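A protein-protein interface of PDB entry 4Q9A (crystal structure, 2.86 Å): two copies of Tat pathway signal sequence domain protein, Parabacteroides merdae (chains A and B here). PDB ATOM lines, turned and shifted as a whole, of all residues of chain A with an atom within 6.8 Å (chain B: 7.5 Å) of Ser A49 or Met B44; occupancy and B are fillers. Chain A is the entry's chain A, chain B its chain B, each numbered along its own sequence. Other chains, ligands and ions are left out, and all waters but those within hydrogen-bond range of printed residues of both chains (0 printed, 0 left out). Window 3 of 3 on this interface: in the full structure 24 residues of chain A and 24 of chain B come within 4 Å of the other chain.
Along chain B the printed residues that touch a printed residue of chain A span positions 42 to 57.
Among the printed residues, 9 pairs touch across the chains.
Ser A49 touches just one residue of chain B: Met B44.
Met B44 touches just these residues of chain A: Met A44, Ser A49 and Leu A212.
No residue of chain B comes within 4 Å of Gly A50.
Of the printed residues of chain A, Leu B53 touches Phe A54 (3.8 Å).
Printed residues of chain A within 4 Å of Asn B42: Leu A212.
Of the printed residues of chain B, Phe A54 touches Leu B53 and Thr B57.
Gly A48 touches none of the printed residues of chain B.
The nearest printed residue of chain A that does not touch Asn B42 is Arg A215 (8.4 Å).
Met A44 touches its own counterpart, Met B44.
Met A44 touches Ser B49, and with the chains exchanged Ser A49 touches Met B44.
Positions printed for both chains: 32, 33, 34, 44, 47, 48, 49, 53 and 72.
Of the 9 pairs that touch across the chains among the printed residues, 3 have their exchanged pair printed and touching as well.
Met B44 touches Met A44.
Ser B49 touches Met A44 (OG to CE, 3.4 Å).
Ser A49 touches Met B44.
CZ of Phe A54 touches CD1 of Leu B53, at 3.8 Å.
Phe A54 touches Thr B57 (CE1 to OG1, 3.7 Å).
Asn B42 touches Leu A212 (O to CD1, 3.4 Å).
Thr B43 touches Leu A212 (C to CD1, 3.7 Å).
Met B44 touches Leu A212.
Leu A212 touches Phe B47 (CD1 to CE2, 3.7 Å).
The side-chain hydroxyl of Thr B43 sits at hydrogen-bond distance from the backbone NH of Gln B46 (3.0 Å).
ND2 of Asn B72 lies within hydrogen-bond range of O of Phe B47 (2.8 Å).
O of Ser A49 sits at hydrogen-bond distance from NH1 of Arg A215 (2.8 Å).
The backbone NH (N) of Ser B49 lies within hydrogen-bond range of the backbone carbonyl oxygen (O) of Cys B32 (3.1 Å).
The side-chain hydroxyl (OG1) of Thr B43 lies within hydrogen-bond range of the side-chain carboxylate (OE1) of Glu B45 (3.2 Å).
The backbone carbonyl oxygen (O) of Cys A32 lies within hydrogen-bond range of the backbone NH (N) of Ser A49 (3.0 Å).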
ATOM      1  N   ILE A  29      -3.732  13.946  13.450  1.00  0.00           N
ATOM      2  CA  ILE A  29      -3.051  12.766  12.870  1.00  0.00           C
ATOM      3  C   ILE A  29      -3.528  12.453  11.435  1.00  0.00           C
ATOM      4  O   ILE A  29      -2.728  12.021  10.589  1.00  0.00           O
ATOM      5  CB  ILE A  29      -3.215  11.519  13.787  1.00  0.00           C
ATOM      6  CG1 ILE A  29      -2.749  11.819  15.222  1.00  0.00           C
ATOM      7  CG2 ILE A  29      -2.480  10.295  13.227  1.00  0.00           C
ATOM      8  CD1 ILE A  29      -3.450  11.090  16.196  1.00  0.00           C
ATOM      9  N   THR A  30      -4.821  12.653  11.174  1.00  0.00           N
ATOM     10  CA  THR A  30      -5.422  12.363   9.879  1.00  0.00           C
ATOM     11  C   THR A  30      -5.168  13.542   8.898  1.00  0.00           C
ATOM     12  O   THR A  30      -4.791  13.284   7.756  1.00  0.00           O
ATOM     13  CB  THR A  30      -6.907  11.988  10.060  1.00  0.00           C
ATOM     14  OG1 THR A  30      -7.047  11.003  11.114  1.00  0.00           O
ATOM     15  CG2 THR A  30      -7.541  11.480   8.771  1.00  0.00           C
ATOM     16  N   ASP A  31      -5.347  14.810   9.347  1.00  0.00           N
ATOM     17  CA  ASP A  31      -5.117  16.053   8.580  1.00  0.00           C
ATOM     18  C   ASP A  31      -3.672  16.110   8.048  1.00  0.00           C
ATOM     19  O   ASP A  31      -3.454  16.064   6.832  1.00  0.00           O
ATOM     20  CB  ASP A  31      -5.395  17.273   9.497  1.00  0.00           C
ATOM     21  CG  ASP A  31      -5.309  18.688   8.934  1.00  0.00           C
ATOM     22  OD1 ASP A  31      -4.735  18.873   7.833  1.00  0.00           O
ATOM     23  OD2 ASP A  31      -5.769  19.616   9.618  1.00  0.00           O
ATOM     24  N   CYS A  32      -2.695  16.217   8.980  1.00  0.00           N
ATOM     25  CA  CYS A  32      -1.256  16.292   8.742  1.00  0.00           C
ATOM     26  C   CYS A  32      -0.914  17.199   7.559  1.00  0.00           C
ATOM     27  O   CYS A  32      -0.376  16.767   6.536  1.00  0.00           O
ATOM     28  CB  CYS A  32      -0.644  14.908   8.578  1.00  0.00           C
ATOM     29  SG  CYS A  32       1.161  14.891   8.738  1.00  0.00           S
ATOM     30  N   GLY A  33      -1.290  18.448   7.713  1.00  0.00           N
ATOM     31  CA  GLY A  33      -1.002  19.496   6.744  1.00  0.00           C
ATOM     32  C   GLY A  33      -1.457  19.302   5.313  1.00  0.00           C
ATOM     33  O   GLY A  33      -0.737  19.699   4.389  1.00  0.00           O
ATOM     34  N   ARG A  34      -2.667  18.745   5.123  1.00  0.00           N
ATOM     35  CA  ARG A  34      -3.266  18.583   3.801  1.00  0.00           C
ATOM     36  C   ARG A  34      -3.803  19.932   3.344  1.00  0.00           C
ATOM     37  O   ARG A  34      -4.165  20.770   4.176  1.00  0.00           O
ATOM     38  CB  ARG A  34      -4.392  17.528   3.831  1.00  0.00           C
ATOM     39  CG  ARG A  34      -5.539  17.867   4.797  1.00  0.00           C
ATOM     40  CD  ARG A  34      -6.774  17.020   4.593  1.00  0.00           C
ATOM     41  NE  ARG A  34      -7.933  17.560   5.299  1.00  0.00           N
ATOM     42  CZ  ARG A  34      -8.878  18.281   4.713  1.00  0.00           C
ATOM     43  NH1 ARG A  34      -8.810  18.545   3.411  1.00  0.00           N
ATOM     44  NH2 ARG A  34      -9.905  18.738   5.418  1.00  0.00           N
ATOM     45  N   MET A  44      -0.970  14.695  -3.540  1.00  0.00           N
ATOM     46  CA  MET A  44      -0.204  15.039  -2.338  1.00  0.00           C
ATOM     47  C   MET A  44      -0.964  16.087  -1.513  1.00  0.00           C
ATOM     48  O   MET A  44      -1.085  15.962  -0.297  1.00  0.00           O
ATOM     49  CB  MET A  44       1.167  15.581  -2.746  1.00  0.00           C
ATOM     50  CG  MET A  44       2.199  14.486  -2.969  1.00  0.00           C
ATOM     51  SD  MET A  44       2.725  13.651  -1.289  1.00  0.00           S
ATOM     52  CE  MET A  44       3.779  15.175  -0.521  1.00  0.00           C
ATOM     53  N   PHE A  47      -4.022  14.429   0.308  1.00  0.00           N
ATOM     54  CA  PHE A  47      -3.618  13.541   1.390  1.00  0.00           C
ATOM     55  C   PHE A  47      -2.833  14.184   2.530  1.00  0.00           C
ATOM     56  O   PHE A  47      -3.022  13.806   3.700  1.00  0.00           O
ATOM     57  CB  PHE A  47      -2.755  12.401   0.811  1.00  0.00           C
ATOM     58  CG  PHE A  47      -3.426  11.543  -0.231  1.00  0.00           C
ATOM     59  CD1 PHE A  47      -4.778  11.225  -0.130  1.00  0.00           C
ATOM     60  CD2 PHE A  47      -2.689  10.972  -1.264  1.00  0.00           C
ATOM     61  CE1 PHE A  47      -5.396  10.429  -1.095  1.00  0.00           C
ATOM     62  CE2 PHE A  47      -3.302  10.154  -2.216  1.00  0.00           C
ATOM     63  CZ  PHE A  47      -4.649   9.882  -2.122  1.00  0.00           C
ATOM     64  N   GLY A  48      -1.902  15.062   2.189  1.00  0.00           N
ATOM     65  CA  GLY A  48      -1.007  15.629   3.181  1.00  0.00           C
ATOM     66  C   GLY A  48       0.171  14.693   3.394  1.00  0.00           C
ATOM     67  O   GLY A  48       0.516  13.918   2.490  1.00  0.00           O
ATOM     68  N   SER A  49       0.782  14.726   4.589  1.00  0.00           N
ATOM     69  CA  SER A  49       1.987  13.931   4.839  1.00  0.00           C
ATOM     70  C   SER A  49       1.837  12.833   5.899  1.00  0.00           C
ATOM     71  O   SER A  49       2.853  12.217   6.268  1.00  0.00           O
ATOM     72  CB  SER A  49       3.132  14.857   5.248  1.00  0.00           C
ATOM     73  OG  SER A  49       3.197  16.003   4.414  1.00  0.00           O
ATOM     74  N   GLY A  50       0.612  12.595   6.379  1.00  0.00           N
ATOM     75  CA  GLY A  50       0.357  11.611   7.435  1.00  0.00           C
ATOM     76  C   GLY A  50       0.232  10.180   6.977  1.00  0.00           C
ATOM     77  O   GLY A  50       0.476   9.868   5.804  1.00  0.00           O
ATOM     78  N   TYR A  51      -0.199   9.304   7.908  1.00  0.00           N
ATOM     79  CA  TYR A  51      -0.457   7.881   7.645  1.00  0.00           C
ATOM     80  C   TYR A  51      -1.444   7.727   6.465  1.00  0.00           C
ATOM     81  O   TYR A  51      -1.392   6.717   5.767  1.00  0.00           O
ATOM     82  CB  TYR A  51      -1.010   7.174   8.904  1.00  0.00           C
ATOM     83  CG  TYR A  51      -2.462   7.493   9.215  1.00  0.00           C
ATOM     84  CD1 TYR A  51      -2.805   8.609   9.976  1.00  0.00           C
ATOM     85  CD2 TYR A  51      -3.496   6.684   8.738  1.00  0.00           C
ATOM     86  CE1 TYR A  51      -4.137   8.894  10.281  1.00  0.00           C
ATOM     87  CE2 TYR A  51      -4.835   6.985   9.001  1.00  0.00           C
ATOM     88  CZ  TYR A  51      -5.148   8.096   9.768  1.00  0.00           C
ATOM     89  OH  TYR A  51      -6.459   8.405  10.043  1.00  0.00           O
ATOM     90  N   VAL A  52      -2.335   8.731   6.253  1.00  0.00           N
ATOM     91  CA  VAL A  52      -3.331   8.708   5.177  1.00  0.00           C
ATOM     92  C   VAL A  52      -2.617   8.612   3.820  1.00  0.00           C
ATOM     93  O   VAL A  52      -2.998   7.781   2.995  1.00  0.00           O
ATOM     94  CB  VAL A  52      -4.280   9.924   5.258  1.00  0.00           C
ATOM     95  CG1 VAL A  52      -5.191   9.999   4.044  1.00  0.00           C
ATOM     96  CG2 VAL A  52      -5.097   9.884   6.539  1.00  0.00           C
ATOM     97  N   LEU A  53      -1.550   9.406   3.628  1.00  0.00           N
ATOM     98  CA  LEU A  53      -0.763   9.383   2.402  1.00  0.00           C
ATOM     99  C   LEU A  53      -0.228   7.951   2.136  1.00  0.00           C
ATOM    100  O   LEU A  53      -0.445   7.406   1.055  1.00  0.00           O
ATOM    101  CB  LEU A  53       0.387  10.417   2.502  1.00  0.00           C
ATOM    102  CG  LEU A  53       1.603  10.259   1.582  1.00  0.00           C
ATOM    103  CD1 LEU A  53       1.220  10.441   0.119  1.00  0.00           C
ATOM    104  CD2 LEU A  53       2.694  11.237   1.965  1.00  0.00           C
ATOM    105  N   PHE A  54       0.405   7.340   3.151  1.00  0.00           N
ATOM    106  CA  PHE A  54       1.038   6.031   3.073  1.00  0.00           C
ATOM    107  C   PHE A  54       0.043   4.886   2.903  1.00  0.00           C
ATOM    108  O   PHE A  54       0.389   3.893   2.267  1.00  0.00           O
ATOM    109  CB  PHE A  54       1.948   5.827   4.278  1.00  0.00           C
ATOM    110  CG  PHE A  54       3.064   6.844   4.237  1.00  0.00           C
ATOM    111  CD1 PHE A  54       4.100   6.730   3.308  1.00  0.00           C
ATOM    112  CD2 PHE A  54       3.033   7.967   5.057  1.00  0.00           C
ATOM    113  CE1 PHE A  54       5.100   7.710   3.216  1.00  0.00           C
ATOM    114  CE2 PHE A  54       4.038   8.939   4.982  1.00  0.00           C
ATOM    115  CZ  PHE A  54       5.069   8.801   4.063  1.00  0.00           C
ATOM    116  N   ASN A  72      -9.224  12.944   1.952  1.00  0.00           N
ATOM    117  CA  ASN A  72      -8.876  13.204   3.352  1.00  0.00           C
ATOM    118  C   ASN A  72      -9.639  14.440   3.820  1.00  0.00           C
ATOM    119  O   ASN A  72      -9.564  15.489   3.170  1.00  0.00           O
ATOM    120  CB  ASN A  72      -7.354  13.392   3.519  1.00  0.00           C
ATOM    121  CG  ASN A  72      -6.823  13.598   4.935  1.00  0.00           C
ATOM    122  OD1 ASN A  72      -7.554  13.779   5.924  1.00  0.00           O
ATOM    123  ND2 ASN A  72      -5.501  13.634   5.056  1.00  0.00           N
ATOM    124  N   PRO A 210       2.335  10.784  15.009  1.00  0.00           N
ATOM    125  CA  PRO A 210       3.411   9.927  14.495  1.00  0.00           C
ATOM    126  C   PRO A 210       4.296  10.604  13.453  1.00  0.00           C
ATOM    127  O   PRO A 210       3.814  11.390  12.630  1.00  0.00           O
ATOM    128  CB  PRO A 210       2.650   8.771  13.844  1.00  0.00           C
ATOM    129  CG  PRO A 210       1.367   9.363  13.424  1.00  0.00           C
ATOM    130  CD  PRO A 210       1.028  10.411  14.429  1.00  0.00           C
ATOM    131  N   LEU A 212       7.519   9.825  10.384  1.00  0.00           N
ATOM    132  CA  LEU A 212       7.591   8.936   9.213  1.00  0.00           C
ATOM    133  C   LEU A 212       7.592   7.411   9.541  1.00  0.00           C
ATOM    134  O   LEU A 212       6.780   6.705   8.918  1.00  0.00           O
ATOM    135  CB  LEU A 212       8.766   9.289   8.299  1.00  0.00           C
ATOM    136  CG  LEU A 212       8.692  10.671   7.650  1.00  0.00           C
ATOM    137  CD1 LEU A 212       9.984  11.010   6.942  1.00  0.00           C
ATOM    138  CD2 LEU A 212       7.472  10.801   6.744  1.00  0.00           C
ATOM    139  N   ARG A 215       3.956   6.537  10.767  1.00  0.00           N
ATOM    140  CA  ARG A 215       2.986   6.724   9.686  1.00  0.00           C
ATOM    141  C   ARG A 215       2.908   5.465   8.835  1.00  0.00           C
ATOM    142  O   ARG A 215       1.814   4.927   8.644  1.00  0.00           O
ATOM    143  CB  ARG A 215       3.385   7.938   8.826  1.00  0.00           C
ATOM    144  CG  ARG A 215       3.081   9.253   9.506  1.00  0.00           C
ATOM    145  CD  ARG A 215       3.821  10.385   8.873  1.00  0.00           C
ATOM    146  NE  ARG A 215       3.934  11.488   9.817  1.00  0.00           N
ATOM    147  CZ  ARG A 215       4.320  12.715   9.499  1.00  0.00           C
ATOM    148  NH1 ARG A 215       4.630  13.017   8.243  1.00  0.00           N
ATOM    149  NH2 ARG A 215       4.397  13.656  10.432  1.00  0.00           N
ATOM    150  N   CYS B  32      12.493  14.647  -6.991  1.00  0.00           N
ATOM    151  CA  CYS B  32      11.045  14.866  -6.869  1.00  0.00           C
ATOM    152  C   CYS B  32      10.660  15.942  -5.781  1.00  0.00           C
ATOM    153  O   CYS B  32       9.813  15.707  -4.910  1.00  0.00           O
ATOM    154  CB  CYS B  32      10.300  13.551  -6.666  1.00  0.00           C
ATOM    155  SG  CYS B  32       8.535  13.618  -7.094  1.00  0.00           S
ATOM    156  N   GLY B  33      11.266  17.127  -5.902  1.00  0.00           N
ATOM    157  CA  GLY B  33      11.021  18.289  -5.048  1.00  0.00           C
ATOM    158  C   GLY B  33      11.487  18.221  -3.607  1.00  0.00           C
ATOM    159  O   GLY B  33      10.866  18.832  -2.732  1.00  0.00           O
ATOM    160  N   ARG B  34      12.564  17.467  -3.334  1.00  0.00           N
ATOM    161  CA  ARG B  34      13.147  17.410  -1.999  1.00  0.00           C
ATOM    162  C   ARG B  34      13.790  18.770  -1.659  1.00  0.00           C
ATOM    163  O   ARG B  34      14.250  19.487  -2.569  1.00  0.00           O
ATOM    164  CB  ARG B  34      14.189  16.282  -1.904  1.00  0.00           C
ATOM    165  CG  ARG B  34      15.361  16.420  -2.895  1.00  0.00           C
ATOM    166  CD  ARG B  34      16.682  15.994  -2.319  1.00  0.00           C
ATOM    167  NE  ARG B  34      17.737  16.132  -3.312  1.00  0.00           N
ATOM    168  CZ  ARG B  34      18.878  16.769  -3.097  1.00  0.00           C
ATOM    169  NH1 ARG B  34      19.131  17.315  -1.915  1.00  0.00           N
ATOM    170  NH2 ARG B  34      19.781  16.865  -4.059  1.00  0.00           N
ATOM    171  N   ASP B  35      13.797  19.133  -0.366  1.00  0.00           N
ATOM    172  CA  ASP B  35      14.444  20.370   0.068  1.00  0.00           C
ATOM    173  C   ASP B  35      15.958  20.141   0.010  1.00  0.00           C
ATOM    174  O   ASP B  35      16.506  19.235   0.658  1.00  0.00           O
ATOM    175  CB  ASP B  35      13.960  20.819   1.463  1.00  0.00           C
ATOM    176  CG  ASP B  35      14.683  22.013   2.066  1.00  0.00           C
ATOM    177  OD1 ASP B  35      15.216  22.848   1.294  1.00  0.00           O
ATOM    178  OD2 ASP B  35      14.679  22.138   3.306  1.00  0.00           O
ATOM    179  N   SER B  38      18.032  20.698   3.269  1.00  0.00           N
ATOM    180  CA  SER B  38      17.907  19.770   4.404  1.00  0.00           C
ATOM    181  C   SER B  38      19.240  19.081   4.719  1.00  0.00           C
ATOM    182  O   SER B  38      19.813  18.374   3.869  1.00  0.00           O
ATOM    183  CB  SER B  38      16.824  18.727   4.155  1.00  0.00           C
ATOM    184  OG  SER B  38      16.543  18.045   5.363  1.00  0.00           O
ATOM    185  N   ARG B  40      19.458  17.280   7.669  1.00  0.00           N
ATOM    186  CA  ARG B  40      18.977  16.183   8.503  1.00  0.00           C
ATOM    187  C   ARG B  40      18.489  15.013   7.685  1.00  0.00           C
ATOM    188  O   ARG B  40      17.780  15.220   6.696  1.00  0.00           O
ATOM    189  CB  ARG B  40      17.802  16.668   9.368  1.00  0.00           C
ATOM    190  CG  ARG B  40      18.122  17.762  10.371  1.00  0.00           C
ATOM    191  CD  ARG B  40      17.238  17.640  11.605  1.00  0.00           C
ATOM    192  NE  ARG B  40      15.825  17.877  11.313  1.00  0.00           N
ATOM    193  CZ  ARG B  40      14.815  17.409  12.045  1.00  0.00           C
ATOM    194  NH1 ARG B  40      15.053  16.662  13.121  1.00  0.00           N
ATOM    195  NH2 ARG B  40      13.560  17.676  11.704  1.00  0.00           N
ATOM    196  N   CYS B  41      18.776  13.785   8.149  1.00  0.00           N
ATOM    197  CA  CYS B  41      18.269  12.581   7.517  1.00  0.00           C
ATOM    198  C   CYS B  41      16.830  12.361   7.975  1.00  0.00           C
ATOM    199  O   CYS B  41      16.333  13.059   8.866  1.00  0.00           O
ATOM    200  CB  CYS B  41      19.146  11.380   7.862  1.00  0.00           C
ATOM    201  SG  CYS B  41      19.250  11.018   9.634  1.00  0.00           S
ATOM    202  N   ASN B  42      16.176  11.364   7.360  1.00  0.00           N
ATOM    203  CA  ASN B  42      14.877  10.803   7.683  1.00  0.00           C
ATOM    204  C   ASN B  42      13.733  11.821   7.882  1.00  0.00           C
ATOM    205  O   ASN B  42      12.860  11.576   8.722  1.00  0.00           O
ATOM    206  CB  ASN B  42      15.015   9.888   8.913  1.00  0.00           C
ATOM    207  CG  ASN B  42      16.117   8.862   8.772  1.00  0.00           C
ATOM    208  OD1 ASN B  42      16.572   8.547   7.665  1.00  0.00           O
ATOM    209  ND2 ASN B  42      16.568   8.313   9.889  1.00  0.00           N
ATOM    210  N   THR B  43      13.679  12.893   7.063  1.00  0.00           N
ATOM    211  CA  THR B  43      12.572  13.871   7.105  1.00  0.00           C
ATOM    212  C   THR B  43      11.889  13.980   5.727  1.00  0.00           C
ATOM    213  O   THR B  43      12.477  13.592   4.715  1.00  0.00           O
ATOM    214  CB  THR B  43      13.012  15.287   7.580  1.00  0.00           C
ATOM    215  OG1 THR B  43      13.725  15.995   6.555  1.00  0.00           O
ATOM    216  CG2 THR B  43      13.757  15.294   8.911  1.00  0.00           C
ATOM    217  N   MET B  44      10.679  14.574   5.688  1.00  0.00           N
ATOM    218  CA  MET B  44       9.937  14.864   4.451  1.00  0.00           C
ATOM    219  C   MET B  44      10.770  15.766   3.543  1.00  0.00           C
ATOM    220  O   MET B  44      10.885  15.513   2.344  1.00  0.00           O
ATOM    221  CB  MET B  44       8.604  15.555   4.778  1.00  0.00           C
ATOM    222  CG  MET B  44       7.480  14.602   5.166  1.00  0.00           C
ATOM    223  SD  MET B  44       6.791  13.669   3.621  1.00  0.00           S
ATOM    224  CE  MET B  44       5.987  15.198   2.608  1.00  0.00           C
ATOM    225  N   GLU B  45      11.386  16.803   4.147  1.00  0.00           N
ATOM    226  CA  GLU B  45      12.271  17.784   3.523  1.00  0.00           C
ATOM    227  C   GLU B  45      13.473  17.094   2.888  1.00  0.00           C
ATOM    228  O   GLU B  45      13.925  17.520   1.826  1.00  0.00           O
ATOM    229  CB  GLU B  45      12.762  18.821   4.566  1.00  0.00           C
ATOM    230  CG  GLU B  45      11.678  19.670   5.225  1.00  0.00           C
ATOM    231  CD  GLU B  45      10.824  19.021   6.303  1.00  0.00           C
ATOM    232  OE1 GLU B  45      11.299  18.093   7.000  1.00  0.00           O
ATOM    233  OE2 GLU B  45       9.670  19.477   6.469  1.00  0.00           O
ATOM    234  N   GLN B  46      14.004  16.032   3.543  1.00  0.00           N
ATOM    235  CA  GLN B  46      15.188  15.319   3.058  1.00  0.00           C
ATOM    236  C   GLN B  46      14.848  14.480   1.827  1.00  0.00           C
ATOM    237  O   GLN B  46      15.567  14.535   0.819  1.00  0.00           O
ATOM    238  CB  GLN B  46      15.807  14.456   4.172  1.00  0.00           C
ATOM    239  CG  GLN B  46      17.052  13.630   3.777  1.00  0.00           C
ATOM    240  CD  GLN B  46      18.288  14.394   3.321  1.00  0.00           C
ATOM    241  OE1 GLN B  46      18.875  14.100   2.279  1.00  0.00           O
ATOM    242  NE2 GLN B  46      18.767  15.334   4.114  1.00  0.00           N
ATOM    243  N   PHE B  47      13.723  13.750   1.904  1.00  0.00           N
ATOM    244  CA  PHE B  47      13.261  12.790   0.908  1.00  0.00           C
ATOM    245  C   PHE B  47      12.524  13.374  -0.288  1.00  0.00           C
ATOM    246  O   PHE B  47      12.685  12.871  -1.411  1.00  0.00           O
ATOM    247  CB  PHE B  47      12.332  11.772   1.583  1.00  0.00           C
ATOM    248  CG  PHE B  47      12.948  10.972   2.711  1.00  0.00           C
ATOM    249  CD1 PHE B  47      14.274  10.549   2.648  1.00  0.00           C
ATOM    250  CD2 PHE B  47      12.183  10.568   3.796  1.00  0.00           C
ATOM    251  CE1 PHE B  47      14.845   9.827   3.696  1.00  0.00           C
ATOM    252  CE2 PHE B  47      12.751   9.819   4.829  1.00  0.00           C
ATOM    253  CZ  PHE B  47      14.074   9.445   4.766  1.00  0.00           C
ATOM    254  N   GLY B  48      11.664  14.349  -0.038  1.00  0.00           N
ATOM    255  CA  GLY B  48      10.811  14.888  -1.082  1.00  0.00           C
ATOM    256  C   GLY B  48       9.564  14.042  -1.217  1.00  0.00           C
ATOM    257  O   GLY B  48       9.157  13.385  -0.252  1.00  0.00           O
ATOM    258  N   SER B  49       8.961  14.015  -2.410  1.00  0.00           N
ATOM    259  CA  SER B  49       7.694  13.313  -2.618  1.00  0.00           C
ATOM    260  C   SER B  49       7.766  12.111  -3.578  1.00  0.00           C
ATOM    261  O   SER B  49       6.717  11.552  -3.903  1.00  0.00           O
ATOM    262  CB  SER B  49       6.646  14.294  -3.133  1.00  0.00           C
ATOM    263  OG  SER B  49       6.662  15.496  -2.380  1.00  0.00           O
ATOM    264  N   LEU B  53      10.874   8.667  -0.932  1.00  0.00           N
ATOM    265  CA  LEU B  53      10.095   8.826   0.292  1.00  0.00           C
ATOM    266  C   LEU B  53       9.446   7.474   0.703  1.00  0.00           C
ATOM    267  O   LEU B  53       9.623   7.025   1.841  1.00  0.00           O
ATOM    268  CB  LEU B  53       9.029   9.928   0.088  1.00  0.00           C
ATOM    269  CG  LEU B  53       7.812   9.975   1.019  1.00  0.00           C
ATOM    270  CD1 LEU B  53       8.209  10.271   2.460  1.00  0.00           C
ATOM    271  CD2 LEU B  53       6.815  10.990   0.529  1.00  0.00           C
ATOM    272  N   THR B  57      10.566   5.181   4.046  1.00  0.00           N
ATOM    273  CA  THR B  57       9.610   4.913   5.112  1.00  0.00           C
ATOM    274  C   THR B  57       9.485   3.406   5.360  1.00  0.00           C
ATOM    275  O   THR B  57       9.389   2.991   6.523  1.00  0.00           O
ATOM    276  CB  THR B  57       8.273   5.589   4.824  1.00  0.00           C
ATOM    277  OG1 THR B  57       7.849   5.255   3.499  1.00  0.00           O
ATOM    278  CG2 THR B  57       8.347   7.106   4.972  1.00  0.00           C
ATOM    279  N   ASN B  72      18.832  11.724   0.432  1.00  0.00           N
ATOM    280  CA  ASN B  72      18.484  11.859  -0.989  1.00  0.00           C
ATOM    281  C   ASN B  72      19.329  12.987  -1.596  1.00  0.00           C
ATOM    282  O   ASN B  72      19.333  14.109  -1.055  1.00  0.00           O
ATOM    283  CB  ASN B  72      16.960  12.131  -1.177  1.00  0.00           C
ATOM    284  CG  ASN B  72      16.434  12.261  -2.617  1.00  0.00           C
ATOM    285  OD1 ASN B  72      17.163  12.278  -3.621  1.00  0.00           O
ATOM    286  ND2 ASN B  72      15.133  12.400  -2.741  1.00  0.00           N
